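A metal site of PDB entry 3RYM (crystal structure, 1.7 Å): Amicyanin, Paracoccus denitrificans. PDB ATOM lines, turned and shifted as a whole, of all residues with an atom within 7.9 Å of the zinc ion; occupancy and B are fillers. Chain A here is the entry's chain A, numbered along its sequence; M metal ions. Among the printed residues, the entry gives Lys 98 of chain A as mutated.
A ring nitrogen (NE2) of His 53 sits close to the backbone carbonyl oxygen (O) of Met 51. NE2 of His 95 is in hydrogen-bond range of SD of Met 51. SG of Cys 92 sits close to N of Asn 54. The backbone NH of Cys 92 lies within hydrogen-bond range of the side-chain hydroxyl of Tyr 30, 3.1 Å away.
The nearest printed residue that does not touch the zinc ion is Pro 52 (4.4 Å).
The zinc ion is bound by a ring nitrogen (ND1) of His 53, the side-chain amino group (NZ) of Lys 98, a ring nitrogen (ND1) of His 95 and the side-chain sulfur (SG) of Cys 92. The zinc ion has four donor atoms within binding distance.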
ATOM      1  N   ILE A  25     -16.058  -0.963 -25.576  1.00  0.00           N
ATOM      2  CA  ILE A  25     -14.914  -0.225 -25.053  1.00  0.00           C
ATOM      3  C   ILE A  25     -13.718  -1.168 -25.001  1.00  0.00           C
ATOM      4  O   ILE A  25     -13.773  -2.223 -24.382  1.00  0.00           O
ATOM      5  CB  ILE A  25     -15.169   0.337 -23.674  1.00  0.00           C
ATOM      6  CG1 ILE A  25     -16.488   1.139 -23.645  1.00  0.00           C
ATOM      7  CG2 ILE A  25     -14.018   1.278 -23.250  1.00  0.00           C
ATOM      8  CD1 ILE A  25     -16.839   1.670 -22.279  1.00  0.00           C
ATOM      9  N   ALA A  26     -12.680  -0.690 -25.662  1.00  0.00           N
ATOM     10  CA  ALA A  26     -11.401  -1.344 -25.702  1.00  0.00           C
ATOM     11  C   ALA A  26     -10.337  -0.458 -25.065  1.00  0.00           C
ATOM     12  O   ALA A  26     -10.523   0.696 -24.799  1.00  0.00           O
ATOM     13  CB  ALA A  26     -11.023  -1.607 -27.154  1.00  0.00           C
ATOM     14  N   LYS A  27      -9.181  -1.040 -24.866  1.00  0.00           N
ATOM     15  CA  LYS A  27      -8.105  -0.265 -24.312  1.00  0.00           C
ATOM     16  C   LYS A  27      -7.799   0.966 -25.084  1.00  0.00           C
ATOM     17  O   LYS A  27      -7.561   2.012 -24.692  1.00  0.00           O
ATOM     18  CB  LYS A  27      -6.846  -1.121 -24.191  1.00  0.00           C
ATOM     19  CG  LYS A  27      -5.721  -0.384 -23.585  1.00  0.00           C
ATOM     20  CD  LYS A  27      -4.308  -1.099 -23.639  1.00  0.00           C
ATOM     21  CE  LYS A  27      -3.249  -0.317 -22.920  1.00  0.00           C
ATOM     22  NZ  LYS A  27      -3.377  -0.253 -21.557  1.00  0.00           N
ATOM     23  N   MET A  28      -7.635   0.764 -26.325  1.00  0.00           N
ATOM     24  CA  MET A  28      -7.078   1.826 -27.027  1.00  0.00           C
ATOM     25  C   MET A  28      -8.078   2.762 -27.669  1.00  0.00           C
ATOM     26  O   MET A  28      -7.702   3.692 -28.335  1.00  0.00           O
ATOM     27  CB  MET A  28      -6.224   1.214 -28.130  1.00  0.00           C
ATOM     28  CG  MET A  28      -5.007   0.501 -27.666  1.00  0.00           C
ATOM     29  SD  MET A  28      -3.914   1.576 -26.739  1.00  0.00           S
ATOM     30  CE  MET A  28      -3.358   2.682 -27.994  1.00  0.00           C
ATOM     31  N   LYS A  29      -9.343   2.414 -27.565  1.00  0.00           N
ATOM     32  CA  LYS A  29     -10.382   3.204 -28.185  1.00  0.00           C
ATOM     33  C   LYS A  29     -11.762   2.693 -27.869  1.00  0.00           C
ATOM     34  O   LYS A  29     -11.920   1.614 -27.441  1.00  0.00           O
ATOM     35  CB  LYS A  29     -10.211   3.220 -29.706  1.00  0.00           C
ATOM     36  CG  LYS A  29     -10.313   1.815 -30.381  1.00  0.00           C
ATOM     37  CD  LYS A  29     -10.700   1.962 -31.857  1.00  0.00           C
ATOM     38  CE  LYS A  29     -10.512   0.670 -32.614  1.00  0.00           C
ATOM     39  NZ  LYS A  29     -10.496   0.849 -34.088  1.00  0.00           N
ATOM     40  N   TYR A  30     -12.753   3.574 -27.976  1.00  0.00           N
ATOM     41  CA  TYR A  30     -14.105   3.119 -28.132  1.00  0.00           C
ATOM     42  C   TYR A  30     -14.115   2.550 -29.541  1.00  0.00           C
ATOM     43  O   TYR A  30     -13.641   3.193 -30.479  1.00  0.00           O
ATOM     44  CB  TYR A  30     -15.060   4.339 -28.001  1.00  0.00           C
ATOM     45  CG  TYR A  30     -15.085   4.953 -26.626  1.00  0.00           C
ATOM     46  CD1 TYR A  30     -15.758   4.331 -25.570  1.00  0.00           C
ATOM     47  CD2 TYR A  30     -14.452   6.169 -26.375  1.00  0.00           C
ATOM     48  CE1 TYR A  30     -15.790   4.903 -24.318  1.00  0.00           C
ATOM     49  CE2 TYR A  30     -14.492   6.743 -25.134  1.00  0.00           C
ATOM     50  CZ  TYR A  30     -15.135   6.106 -24.094  1.00  0.00           C
ATOM     51  OH  TYR A  30     -15.144   6.718 -22.864  1.00  0.00           O
ATOM     52  N   ASN A  47     -18.118  -2.594 -21.685  1.00  0.00           N
ATOM     53  CA  ASN A  47     -16.694  -2.737 -21.400  1.00  0.00           C
ATOM     54  C   ASN A  47     -16.217  -4.167 -21.681  1.00  0.00           C
ATOM     55  O   ASN A  47     -16.669  -5.127 -21.059  1.00  0.00           O
ATOM     56  CB  ASN A  47     -16.367  -2.360 -19.957  1.00  0.00           C
ATOM     57  CG  ASN A  47     -14.874  -2.318 -19.705  1.00  0.00           C
ATOM     58  OD1 ASN A  47     -14.096  -2.509 -20.646  1.00  0.00           O
ATOM     59  ND2 ASN A  47     -14.483  -2.053 -18.479  1.00  0.00           N
ATOM     60  N   GLU A  49     -12.906  -5.008 -21.537  1.00  0.00           N
ATOM     61  CA  GLU A  49     -11.604  -5.156 -20.868  1.00  0.00           C
ATOM     62  C   GLU A  49     -11.786  -5.310 -19.360  1.00  0.00           C
ATOM     63  O   GLU A  49     -12.792  -4.996 -18.818  1.00  0.00           O
ATOM     64  CB  GLU A  49     -10.694  -3.933 -21.064  1.00  0.00           C
ATOM     65  CG  GLU A  49     -10.529  -3.303 -22.373  1.00  0.00           C
ATOM     66  CD  GLU A  49      -9.703  -4.110 -23.317  1.00  0.00           C
ATOM     67  OE1 GLU A  49      -9.268  -5.153 -22.939  1.00  0.00           O
ATOM     68  OE2 GLU A  49      -9.500  -3.736 -24.451  1.00  0.00           O
ATOM     69  N   MET A  51      -9.817  -3.659 -17.097  1.00  0.00           N
ATOM     70  CA  MET A  51      -9.683  -2.282 -16.664  1.00  0.00           C
ATOM     71  C   MET A  51     -11.035  -1.583 -16.720  1.00  0.00           C
ATOM     72  O   MET A  51     -11.688  -1.640 -17.766  1.00  0.00           O
ATOM     73  CB  MET A  51      -8.706  -1.551 -17.583  1.00  0.00           C
ATOM     74  CG  MET A  51      -8.652  -0.054 -17.371  1.00  0.00           C
ATOM     75  SD  MET A  51      -7.738   0.418 -15.922  1.00  0.00           S
ATOM     76  CE  MET A  51      -6.073  -0.014 -16.407  1.00  0.00           C
ATOM     77  N   PRO A  52     -11.458  -0.938 -15.625  1.00  0.00           N
ATOM     78  CA  PRO A  52     -12.733  -0.225 -15.695  1.00  0.00           C
ATOM     79  C   PRO A  52     -12.665   0.986 -16.607  1.00  0.00           C
ATOM     80  O   PRO A  52     -11.654   1.672 -16.652  1.00  0.00           O
ATOM     81  CB  PRO A  52     -12.978   0.213 -14.261  1.00  0.00           C
ATOM     82  CG  PRO A  52     -12.137  -0.710 -13.416  1.00  0.00           C
ATOM     83  CD  PRO A  52     -10.926  -0.968 -14.253  1.00  0.00           C
ATOM     84  N   HIS A  53     -13.757   1.213 -17.330  1.00  0.00           N
ATOM     85  CA  HIS A  53     -13.893   2.433 -18.141  1.00  0.00           C
ATOM     86  C   HIS A  53     -15.273   3.028 -17.950  1.00  0.00           C
ATOM     87  O   HIS A  53     -16.153   2.394 -17.390  1.00  0.00           O
ATOM     88  CB  HIS A  53     -13.741   2.091 -19.634  1.00  0.00           C
ATOM     89  CG  HIS A  53     -12.443   1.429 -19.973  1.00  0.00           C
ATOM     90  ND1 HIS A  53     -11.273   2.129 -20.125  1.00  0.00           N
ATOM     91  CD2 HIS A  53     -12.135   0.120 -20.164  1.00  0.00           C
ATOM     92  CE1 HIS A  53     -10.287   1.292 -20.436  1.00  0.00           C
ATOM     93  NE2 HIS A  53     -10.790   0.060 -20.465  1.00  0.00           N
ATOM     94  N   ASN A  54     -15.475   4.223 -18.474  1.00  0.00           N
ATOM     95  CA  ASN A  54     -16.811   4.815 -18.448  1.00  0.00           C
ATOM     96  C   ASN A  54     -17.036   5.680 -19.659  1.00  0.00           C
ATOM     97  O   ASN A  54     -16.236   5.656 -20.595  1.00  0.00           O
ATOM     98  CB  ASN A  54     -17.114   5.578 -17.147  1.00  0.00           C
ATOM     99  CG  ASN A  54     -16.406   6.940 -17.092  1.00  0.00           C
ATOM    100  OD1 ASN A  54     -15.381   7.125 -17.764  1.00  0.00           O
ATOM    101  ND2 ASN A  54     -16.908   7.857 -16.282  1.00  0.00           N
ATOM    102  N   VAL A  55     -18.145   6.398 -19.657  1.00  0.00           N
ATOM    103  CA  VAL A  55     -18.382   7.471 -20.625  1.00  0.00           C
ATOM    104  C   VAL A  55     -18.720   8.717 -19.855  1.00  0.00           C
ATOM    105  O   VAL A  55     -19.474   8.665 -18.866  1.00  0.00           O
ATOM    106  CB  VAL A  55     -19.493   7.139 -21.668  1.00  0.00           C
ATOM    107  CG1 VAL A  55     -19.071   5.986 -22.567  1.00  0.00           C
ATOM    108  CG2 VAL A  55     -20.817   6.848 -20.967  1.00  0.00           C
ATOM    109  N   MET A  71     -18.557   3.823 -13.385  1.00  0.00           N
ATOM    110  CA  MET A  71     -17.467   3.019 -13.892  1.00  0.00           C
ATOM    111  C   MET A  71     -17.940   1.600 -14.180  1.00  0.00           C
ATOM    112  O   MET A  71     -18.631   0.994 -13.399  1.00  0.00           O
ATOM    113  CB  MET A  71     -16.328   3.006 -12.877  1.00  0.00           C
ATOM    114  CG  MET A  71     -15.682   4.390 -12.693  1.00  0.00           C
ATOM    115  SD  MET A  71     -14.954   5.076 -14.204  1.00  0.00           S
ATOM    116  CE  MET A  71     -13.627   3.957 -14.549  1.00  0.00           C
ATOM    117  N   HIS A  91     -15.747  11.216 -23.230  1.00  0.00           N
ATOM    118  CA  HIS A  91     -14.440  10.571 -23.012  1.00  0.00           C
ATOM    119  C   HIS A  91     -14.489   9.673 -21.814  1.00  0.00           C
ATOM    120  O   HIS A  91     -15.491   9.602 -21.091  1.00  0.00           O
ATOM    121  CB  HIS A  91     -13.348  11.636 -22.831  1.00  0.00           C
ATOM    122  CG  HIS A  91     -13.484  12.415 -21.555  1.00  0.00           C
ATOM    123  ND1 HIS A  91     -14.257  13.545 -21.460  1.00  0.00           N
ATOM    124  CD2 HIS A  91     -12.976  12.209 -20.321  1.00  0.00           C
ATOM    125  CE1 HIS A  91     -14.205  14.017 -20.232  1.00  0.00           C
ATOM    126  NE2 HIS A  91     -13.426  13.213 -19.515  1.00  0.00           N
ATOM    127  N   CYS A  92     -13.393   8.957 -21.567  1.00  0.00           N
ATOM    128  CA  CYS A  92     -13.302   8.068 -20.402  1.00  0.00           C
ATOM    129  C   CYS A  92     -12.621   8.787 -19.252  1.00  0.00           C
ATOM    130  O   CYS A  92     -11.484   9.248 -19.367  1.00  0.00           O
ATOM    131  CB  CYS A  92     -12.502   6.822 -20.786  1.00  0.00           C
ATOM    132  SG  CYS A  92     -12.447   5.636 -19.475  1.00  0.00           S
ATOM    133  N   THR A  93     -13.301   8.876 -18.116  1.00  0.00           N
ATOM    134  CA  THR A  93     -12.812   9.742 -17.038  1.00  0.00           C
ATOM    135  C   THR A  93     -11.374   9.475 -16.595  1.00  0.00           C
ATOM    136  O   THR A  93     -10.552  10.385 -16.516  1.00  0.00           O
ATOM    137  CB  THR A  93     -13.777   9.721 -15.841  1.00  0.00           C
ATOM    138  OG1 THR A  93     -15.069  10.142 -16.255  1.00  0.00           O
ATOM    139  CG2 THR A  93     -13.265  10.644 -14.728  1.00  0.00           C
ATOM    140  N   PRO A  94     -11.056   8.204 -16.288  1.00  0.00           N
ATOM    141  CA  PRO A  94      -9.678   7.906 -15.846  1.00  0.00           C
ATOM    142  C   PRO A  94      -8.680   7.904 -16.985  1.00  0.00           C
ATOM    143  O   PRO A  94      -7.463   7.986 -16.723  1.00  0.00           O
ATOM    144  CB  PRO A  94      -9.805   6.502 -15.274  1.00  0.00           C
ATOM    145  CG  PRO A  94     -10.994   5.914 -15.954  1.00  0.00           C
ATOM    146  CD  PRO A  94     -11.949   7.061 -16.135  1.00  0.00           C
ATOM    147  N   HIS A  95      -9.147   7.789 -18.221  1.00  0.00           N
ATOM    148  CA  HIS A  95      -8.274   7.744 -19.400  1.00  0.00           C
ATOM    149  C   HIS A  95      -8.797   8.758 -20.415  1.00  0.00           C
ATOM    150  O   HIS A  95      -9.260   8.369 -21.492  1.00  0.00           O
ATOM    151  CB  HIS A  95      -8.297   6.345 -20.014  1.00  0.00           C
ATOM    152  CG  HIS A  95      -8.197   5.236 -19.005  1.00  0.00           C
ATOM    153  ND1 HIS A  95      -9.116   4.219 -18.940  1.00  0.00           N
ATOM    154  CD2 HIS A  95      -7.294   4.997 -18.021  1.00  0.00           C
ATOM    155  CE1 HIS A  95      -8.810   3.399 -17.950  1.00  0.00           C
ATOM    156  NE2 HIS A  95      -7.693   3.844 -17.375  1.00  0.00           N
ATOM    157  N   PRO A  96      -8.692  10.048 -20.093  1.00  0.00           N
ATOM    158  CA  PRO A  96      -9.412  11.124 -20.793  1.00  0.00           C
ATOM    159  C   PRO A  96      -8.977  11.394 -22.197  1.00  0.00           C
ATOM    160  O   PRO A  96      -9.594  12.080 -22.964  1.00  0.00           O
ATOM    161  CB  PRO A  96      -9.165  12.340 -19.909  1.00  0.00           C
ATOM    162  CG  PRO A  96      -7.893  12.045 -19.198  1.00  0.00           C
ATOM    163  CD  PRO A  96      -7.927  10.559 -18.935  1.00  0.00           C
ATOM    164  N   PHE A  97      -7.753  11.069 -22.434  1.00  0.00           N
ATOM    165  CA  PHE A  97      -7.371  10.975 -23.788  1.00  0.00           C
ATOM    166  C   PHE A  97      -8.182   9.941 -24.653  1.00  0.00           C
ATOM    167  O   PHE A  97      -8.176   9.993 -25.810  1.00  0.00           O
ATOM    168  CB  PHE A  97      -5.875  10.625 -23.851  1.00  0.00           C
ATOM    169  CG  PHE A  97      -5.547   9.328 -23.141  1.00  0.00           C
ATOM    170  CD1 PHE A  97      -5.603   8.127 -23.801  1.00  0.00           C
ATOM    171  CD2 PHE A  97      -5.176   9.324 -21.809  1.00  0.00           C
ATOM    172  CE1 PHE A  97      -5.298   6.936 -23.152  1.00  0.00           C
ATOM    173  CE2 PHE A  97      -4.871   8.131 -21.171  1.00  0.00           C
ATOM    174  CZ  PHE A  97      -4.945   6.952 -21.847  1.00  0.00           C
ATOM    175  N   LYS A  98      -8.978   9.014 -24.197  1.00  0.00           N
ATOM    176  CA  LYS A  98      -9.845   8.147 -25.046  1.00  0.00           C
ATOM    177  C   LYS A  98     -11.176   8.834 -25.182  1.00  0.00           C
ATOM    178  O   LYS A  98     -11.893   9.101 -24.262  1.00  0.00           O
ATOM    179  CB  LYS A  98     -10.010   6.811 -24.296  1.00  0.00           C
ATOM    180  CG  LYS A  98     -10.860   5.776 -25.036  1.00  0.00           C
ATOM    181  CD  LYS A  98     -10.654   4.375 -24.537  1.00  0.00           C
ATOM    182  CE  LYS A  98     -11.158   4.152 -23.115  1.00  0.00           C
ATOM    183  NZ  LYS A  98     -10.107   4.494 -22.117  1.00  0.00           N
HETATM  184 ZN    ZN M   1     -10.828   4.135 -20.210  1.00  0.00          ZN
